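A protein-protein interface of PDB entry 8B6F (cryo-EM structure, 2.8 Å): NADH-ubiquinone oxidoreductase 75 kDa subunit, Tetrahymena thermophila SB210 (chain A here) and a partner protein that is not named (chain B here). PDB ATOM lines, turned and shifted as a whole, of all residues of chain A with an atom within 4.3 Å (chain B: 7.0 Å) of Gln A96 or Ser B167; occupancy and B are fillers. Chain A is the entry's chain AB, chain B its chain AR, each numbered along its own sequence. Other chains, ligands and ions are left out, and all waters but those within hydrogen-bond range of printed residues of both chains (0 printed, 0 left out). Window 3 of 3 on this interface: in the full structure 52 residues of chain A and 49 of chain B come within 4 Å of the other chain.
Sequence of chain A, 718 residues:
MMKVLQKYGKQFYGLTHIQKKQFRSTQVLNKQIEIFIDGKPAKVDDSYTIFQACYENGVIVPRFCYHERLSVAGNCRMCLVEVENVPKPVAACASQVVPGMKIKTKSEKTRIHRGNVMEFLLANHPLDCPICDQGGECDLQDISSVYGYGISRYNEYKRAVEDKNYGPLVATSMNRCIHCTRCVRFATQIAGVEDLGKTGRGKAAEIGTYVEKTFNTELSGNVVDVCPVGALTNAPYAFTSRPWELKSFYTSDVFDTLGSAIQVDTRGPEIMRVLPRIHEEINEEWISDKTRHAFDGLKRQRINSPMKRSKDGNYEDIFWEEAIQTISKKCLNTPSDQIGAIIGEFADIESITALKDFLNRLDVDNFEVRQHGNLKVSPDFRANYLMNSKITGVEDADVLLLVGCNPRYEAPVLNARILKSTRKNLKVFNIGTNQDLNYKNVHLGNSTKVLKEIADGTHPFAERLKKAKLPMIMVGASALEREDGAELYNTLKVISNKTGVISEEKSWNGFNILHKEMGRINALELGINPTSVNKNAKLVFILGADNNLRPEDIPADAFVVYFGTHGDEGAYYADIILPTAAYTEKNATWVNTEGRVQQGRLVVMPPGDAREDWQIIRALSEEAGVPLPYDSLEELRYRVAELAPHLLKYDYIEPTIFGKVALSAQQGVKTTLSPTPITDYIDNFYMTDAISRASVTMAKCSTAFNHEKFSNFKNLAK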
ATOM      1  N   ASP A  46     -29.694 -27.429  13.481  1.00  0.00           N
ATOM      2  CA  ASP A  46     -29.735 -26.895  14.837  1.00  0.00           C
ATOM      3  C   ASP A  46     -28.360 -26.466  15.336  1.00  0.00           C
ATOM      4  O   ASP A  46     -28.278 -25.623  16.234  1.00  0.00           O
ATOM      5  CB  ASP A  46     -30.335 -27.928  15.789  1.00  0.00           C
ATOM      6  CG  ASP A  46     -29.564 -29.233  15.795  1.00  0.00           C
ATOM      7  OD1 ASP A  46     -28.987 -29.589  14.746  1.00  0.00           O
ATOM      8  OD2 ASP A  46     -29.535 -29.904  16.847  1.00  0.00           O
ATOM      9  N   TYR A  48     -26.336 -24.573  13.943  1.00  0.00           N
ATOM     10  CA  TYR A  48     -26.078 -23.188  13.581  1.00  0.00           C
ATOM     11  C   TYR A  48     -26.427 -22.246  14.725  1.00  0.00           C
ATOM     12  O   TYR A  48     -27.360 -22.483  15.496  1.00  0.00           O
ATOM     13  CB  TYR A  48     -26.890 -22.805  12.345  1.00  0.00           C
ATOM     14  CG  TYR A  48     -26.134 -22.913  11.045  1.00  0.00           C
ATOM     15  CD1 TYR A  48     -25.712 -24.144  10.565  1.00  0.00           C
ATOM     16  CD2 TYR A  48     -25.861 -21.784  10.289  1.00  0.00           C
ATOM     17  CE1 TYR A  48     -25.027 -24.245   9.372  1.00  0.00           C
ATOM     18  CE2 TYR A  48     -25.179 -21.874   9.097  1.00  0.00           C
ATOM     19  CZ  TYR A  48     -24.764 -23.106   8.642  1.00  0.00           C
ATOM     20  OH  TYR A  48     -24.084 -23.197   7.451  1.00  0.00           O
ATOM     21  N   THR A  49     -25.662 -21.166  14.830  1.00  0.00           N
ATOM     22  CA  THR A  49     -26.022 -20.044  15.679  1.00  0.00           C
ATOM     23  C   THR A  49     -26.796 -19.015  14.859  1.00  0.00           C
ATOM     24  O   THR A  49     -26.903 -19.111  13.636  1.00  0.00           O
ATOM     25  CB  THR A  49     -24.780 -19.405  16.303  1.00  0.00           C
ATOM     26  OG1 THR A  49     -23.903 -18.938  15.271  1.00  0.00           O
ATOM     27  CG2 THR A  49     -24.042 -20.405  17.175  1.00  0.00           C
ATOM     28  N   VAL A  72     -15.936 -18.552  21.268  1.00  0.00           N
ATOM     29  CA  VAL A  72     -17.131 -17.717  21.302  1.00  0.00           C
ATOM     30  C   VAL A  72     -17.123 -16.906  22.590  1.00  0.00           C
ATOM     31  O   VAL A  72     -16.975 -17.461  23.684  1.00  0.00           O
ATOM     32  CB  VAL A  72     -18.405 -18.569  21.193  1.00  0.00           C
ATOM     33  CG1 VAL A  72     -19.641 -17.682  21.176  1.00  0.00           C
ATOM     34  CG2 VAL A  72     -18.353 -19.437  19.951  1.00  0.00           C
ATOM     35  N   SER A  95     -25.694 -17.513  20.373  1.00  0.00           N
ATOM     36  CA  SER A  95     -27.039 -18.042  20.548  1.00  0.00           C
ATOM     37  C   SER A  95     -27.374 -19.027  19.440  1.00  0.00           C
ATOM     38  O   SER A  95     -27.241 -18.699  18.258  1.00  0.00           O
ATOM     39  CB  SER A  95     -28.054 -16.900  20.589  1.00  0.00           C
ATOM     40  OG  SER A  95     -27.766 -16.071  21.702  1.00  0.00           O
ATOM     41  N   GLN A  96     -27.810 -20.224  19.821  1.00  0.00           N
ATOM     42  CA  GLN A  96     -28.187 -21.234  18.844  1.00  0.00           C
ATOM     43  C   GLN A  96     -29.613 -21.007  18.358  1.00  0.00           C
ATOM     44  O   GLN A  96     -30.465 -20.482  19.078  1.00  0.00           O
ATOM     45  CB  GLN A  96     -28.068 -22.633  19.447  1.00  0.00           C
ATOM     46  CG  GLN A  96     -26.639 -23.061  19.714  1.00  0.00           C
ATOM     47  CD  GLN A  96     -26.528 -24.528  20.063  1.00  0.00           C
ATOM     48  OE1 GLN A  96     -27.532 -25.229  20.175  1.00  0.00           O
ATOM     49  NE2 GLN A  96     -25.299 -25.001  20.242  1.00  0.00           N
ATOM     50  N   VAL A  97     -29.864 -21.415  17.111  1.00  0.00           N
ATOM     51  CA  VAL A  97     -31.191 -21.249  16.532  1.00  0.00           C
ATOM     52  C   VAL A  97     -32.180 -22.198  17.200  1.00  0.00           C
ATOM     53  O   VAL A  97     -31.821 -23.246  17.748  1.00  0.00           O
ATOM     54  CB  VAL A  97     -31.157 -21.464  15.010  1.00  0.00           C
ATOM     55  CG1 VAL A  97     -30.270 -20.423  14.348  1.00  0.00           C
ATOM     56  CG2 VAL A  97     -30.685 -22.871  14.671  1.00  0.00           C
ATOM     57  N   VAL A  98     -33.453 -21.815  17.147  1.00  0.00           N
ATOM     58  CA  VAL A  98     -34.536 -22.593  17.740  1.00  0.00           C
ATOM     59  C   VAL A  98     -35.630 -22.739  16.690  1.00  0.00           C
ATOM     60  O   VAL A  98     -35.815 -21.829  15.869  1.00  0.00           O
ATOM     61  CB  VAL A  98     -35.066 -21.918  19.016  1.00  0.00           C
ATOM     62  CG1 VAL A  98     -36.134 -22.770  19.680  1.00  0.00           C
ATOM     63  CG2 VAL A  98     -33.924 -21.641  19.983  1.00  0.00           C
ATOM     64  N   MET A 101     -38.148 -19.764  15.230  1.00  0.00           N
ATOM     65  CA  MET A 101     -37.632 -18.484  15.695  1.00  0.00           C
ATOM     66  C   MET A 101     -37.991 -17.381  14.708  1.00  0.00           C
ATOM     67  O   MET A 101     -37.850 -17.545  13.494  1.00  0.00           O
ATOM     68  CB  MET A 101     -36.117 -18.568  15.878  1.00  0.00           C
ATOM     69  CG  MET A 101     -35.486 -17.284  16.392  1.00  0.00           C
ATOM     70  SD  MET A 101     -33.707 -17.430  16.638  1.00  0.00           S
ATOM     71  CE  MET A 101     -33.645 -18.500  18.071  1.00  0.00           C
ATOM     72  N   THR B 164     -17.587 -24.571  10.407  1.00  0.00           N
ATOM     73  CA  THR B 164     -17.300 -25.363  11.593  1.00  0.00           C
ATOM     74  C   THR B 164     -18.369 -25.104  12.643  1.00  0.00           C
ATOM     75  O   THR B 164     -18.928 -24.008  12.726  1.00  0.00           O
ATOM     76  CB  THR B 164     -15.918 -25.038  12.174  1.00  0.00           C
ATOM     77  OG1 THR B 164     -15.820 -23.632  12.431  1.00  0.00           O
ATOM     78  CG2 THR B 164     -14.821 -25.459  11.209  1.00  0.00           C
ATOM     79  N   ARG B 165     -18.645 -26.126  13.446  1.00  0.00           N
ATOM     80  CA  ARG B 165     -19.657 -26.005  14.484  1.00  0.00           C
ATOM     81  C   ARG B 165     -19.203 -25.000  15.534  1.00  0.00           C
ATOM     82  O   ARG B 165     -18.070 -25.060  16.018  1.00  0.00           O
ATOM     83  CB  ARG B 165     -19.929 -27.365  15.123  1.00  0.00           C
ATOM     84  CG  ARG B 165     -21.083 -27.357  16.113  1.00  0.00           C
ATOM     85  CD  ARG B 165     -21.543 -28.770  16.431  1.00  0.00           C
ATOM     86  NE  ARG B 165     -22.700 -28.780  17.316  1.00  0.00           N
ATOM     87  CZ  ARG B 165     -23.385 -29.869  17.642  1.00  0.00           C
ATOM     88  NH1 ARG B 165     -23.061 -31.059  17.162  1.00  0.00           N
ATOM     89  NH2 ARG B 165     -24.421 -29.761  18.469  1.00  0.00           N
ATOM     90  N   LYS B 166     -20.094 -24.075  15.882  1.00  0.00           N
ATOM     91  CA  LYS B 166     -19.795 -22.993  16.810  1.00  0.00           C
ATOM     92  C   LYS B 166     -20.834 -22.999  17.918  1.00  0.00           C
ATOM     93  O   LYS B 166     -22.036 -23.064  17.642  1.00  0.00           O
ATOM     94  CB  LYS B 166     -19.792 -21.641  16.090  1.00  0.00           C
ATOM     95  CG  LYS B 166     -18.781 -20.648  16.631  1.00  0.00           C
ATOM     96  CD  LYS B 166     -17.362 -21.034  16.237  1.00  0.00           C
ATOM     97  CE  LYS B 166     -16.363 -19.976  16.673  1.00  0.00           C
ATOM     98  NZ  LYS B 166     -14.971 -20.345  16.301  1.00  0.00           N
ATOM     99  N   SER B 167     -20.374 -22.933  19.163  1.00  0.00           N
ATOM    100  CA  SER B 167     -21.278 -22.938  20.303  1.00  0.00           C
ATOM    101  C   SER B 167     -20.533 -22.419  21.525  1.00  0.00           C
ATOM    102  O   SER B 167     -19.371 -22.765  21.742  1.00  0.00           O
ATOM    103  CB  SER B 167     -21.825 -24.344  20.570  1.00  0.00           C
ATOM    104  OG  SER B 167     -22.712 -24.348  21.674  1.00  0.00           O
ATOM    105  N   TYR B 168     -21.215 -21.590  22.317  1.00  0.00           N
ATOM    106  CA  TYR B 168     -20.610 -21.052  23.527  1.00  0.00           C
ATOM    107  C   TYR B 168     -20.389 -22.125  24.585  1.00  0.00           C
ATOM    108  O   TYR B 168     -19.531 -21.951  25.456  1.00  0.00           O
ATOM    109  CB  TYR B 168     -21.481 -19.932  24.097  1.00  0.00           C
ATOM    110  CG  TYR B 168     -20.843 -19.200  25.254  1.00  0.00           C
ATOM    111  CD1 TYR B 168     -20.032 -18.098  25.034  1.00  0.00           C
ATOM    112  CD2 TYR B 168     -21.051 -19.611  26.564  1.00  0.00           C
ATOM    113  CE1 TYR B 168     -19.442 -17.424  26.083  1.00  0.00           C
ATOM    114  CE2 TYR B 168     -20.464 -18.942  27.622  1.00  0.00           C
ATOM    115  CZ  TYR B 168     -19.660 -17.850  27.372  1.00  0.00           C
ATOM    116  OH  TYR B 168     -19.069 -17.173  28.412  1.00  0.00           O
ATOM    117  N   ALA B 169     -21.142 -23.224  24.531  1.00  0.00           N
ATOM    118  CA  ALA B 169     -20.968 -24.297  25.502  1.00  0.00           C
ATOM    119  C   ALA B 169     -19.606 -24.964  25.385  1.00  0.00           C
ATOM    120  O   ALA B 169     -19.152 -25.590  26.349  1.00  0.00           O
ATOM    121  CB  ALA B 169     -22.072 -25.342  25.335  1.00  0.00           C
ATOM    122  N   ASP B 170     -18.944 -24.846  24.231  1.00  0.00           N
ATOM    123  CA  ASP B 170     -17.622 -25.434  24.067  1.00  0.00           C
ATOM    124  C   ASP B 170     -16.588 -24.783  24.976  1.00  0.00           C
ATOM    125  O   ASP B 170     -15.530 -25.376  25.211  1.00  0.00           O
ATOM    126  CB  ASP B 170     -17.174 -25.317  22.610  1.00  0.00           C
ATOM    127  CG  ASP B 170     -18.131 -25.995  21.652  1.00  0.00           C
ATOM    128  OD1 ASP B 170     -18.769 -26.990  22.055  1.00  0.00           O
ATOM    129  OD2 ASP B 170     -18.247 -25.534  20.498  1.00  0.00           O
ATOM    130  N   ASN B 171     -16.865 -23.581  25.485  1.00  0.00           N
ATOM    131  CA  ASN B 171     -15.938 -22.948  26.418  1.00  0.00           C
ATOM    132  C   ASN B 171     -15.810 -23.765  27.698  1.00  0.00           C
ATOM    133  O   ASN B 171     -14.712 -23.896  28.252  1.00  0.00           O
ATOM    134  CB  ASN B 171     -16.401 -21.525  26.730  1.00  0.00           C
ATOM    135  CG  ASN B 171     -16.404 -20.629  25.506  1.00  0.00           C
ATOM    136  OD1 ASN B 171     -16.373 -21.108  24.373  1.00  0.00           O
ATOM    137  ND2 ASN B 171     -16.445 -19.322  25.729  1.00  0.00           N
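Of the 9 printed residues of chain A, 3 touch a printed residue of chain B.
Along chain A the printed residues that touch a printed residue of chain B span positions 49 to 96.
Of the 8 printed residues of chain B, 4 touch a printed residue of chain A.
The side-chain amide oxygen (OD1) of Asn B171 lies close to the backbone carbonyl oxygen (O) of Tyr B168 (3.4 Å).
The side-chain hydroxyl (OG) of Ser B167 lies close to the backbone NH (N) of Ala B169, at 3.4 Å.
Among the printed residues, pairs that only touch across the chains: Thr A49 with Lys B166 (3.4 Å), Val A72 with Lys B166 (3.6 Å), Val A72 with Ser B167 (3.9 Å) and Val A72 with Tyr B168 (3.4 Å).
The backbone carbonyl oxygen (O) of Val A72 sits at hydrogen-bond distance from the side-chain amide nitrogen (ND2) of Asn B171 (2.8 Å).
NE2 of Gln A96 lies within hydrogen-bond range of OG of Ser B167 (3.0 Å).
Of chain B, only Ser B167 (3.0 Å) comes within 4 Å of Gln A96.
Printed residues of chain A within 4 Å of Asn B171: Val A72 (2.8 Å).
Printed residues of chain A within 4 Å of Tyr B168: Val A72 (3.4 Å).
Of the printed residues of chain B, Val A72 touches Lys B166, Ser B167, Tyr B168 and Asn B171.
Ala B169 touches none of the printed residues of chain A.
Asp B170 touches none of the printed residues of chain A.
The nearest printed residue of chain A that does not touch Ser B167 is Thr A49 (4.9 Å).
The nearest printed residue of chain B that does not touch Thr A49 is Ser B167 (4.9 Å).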
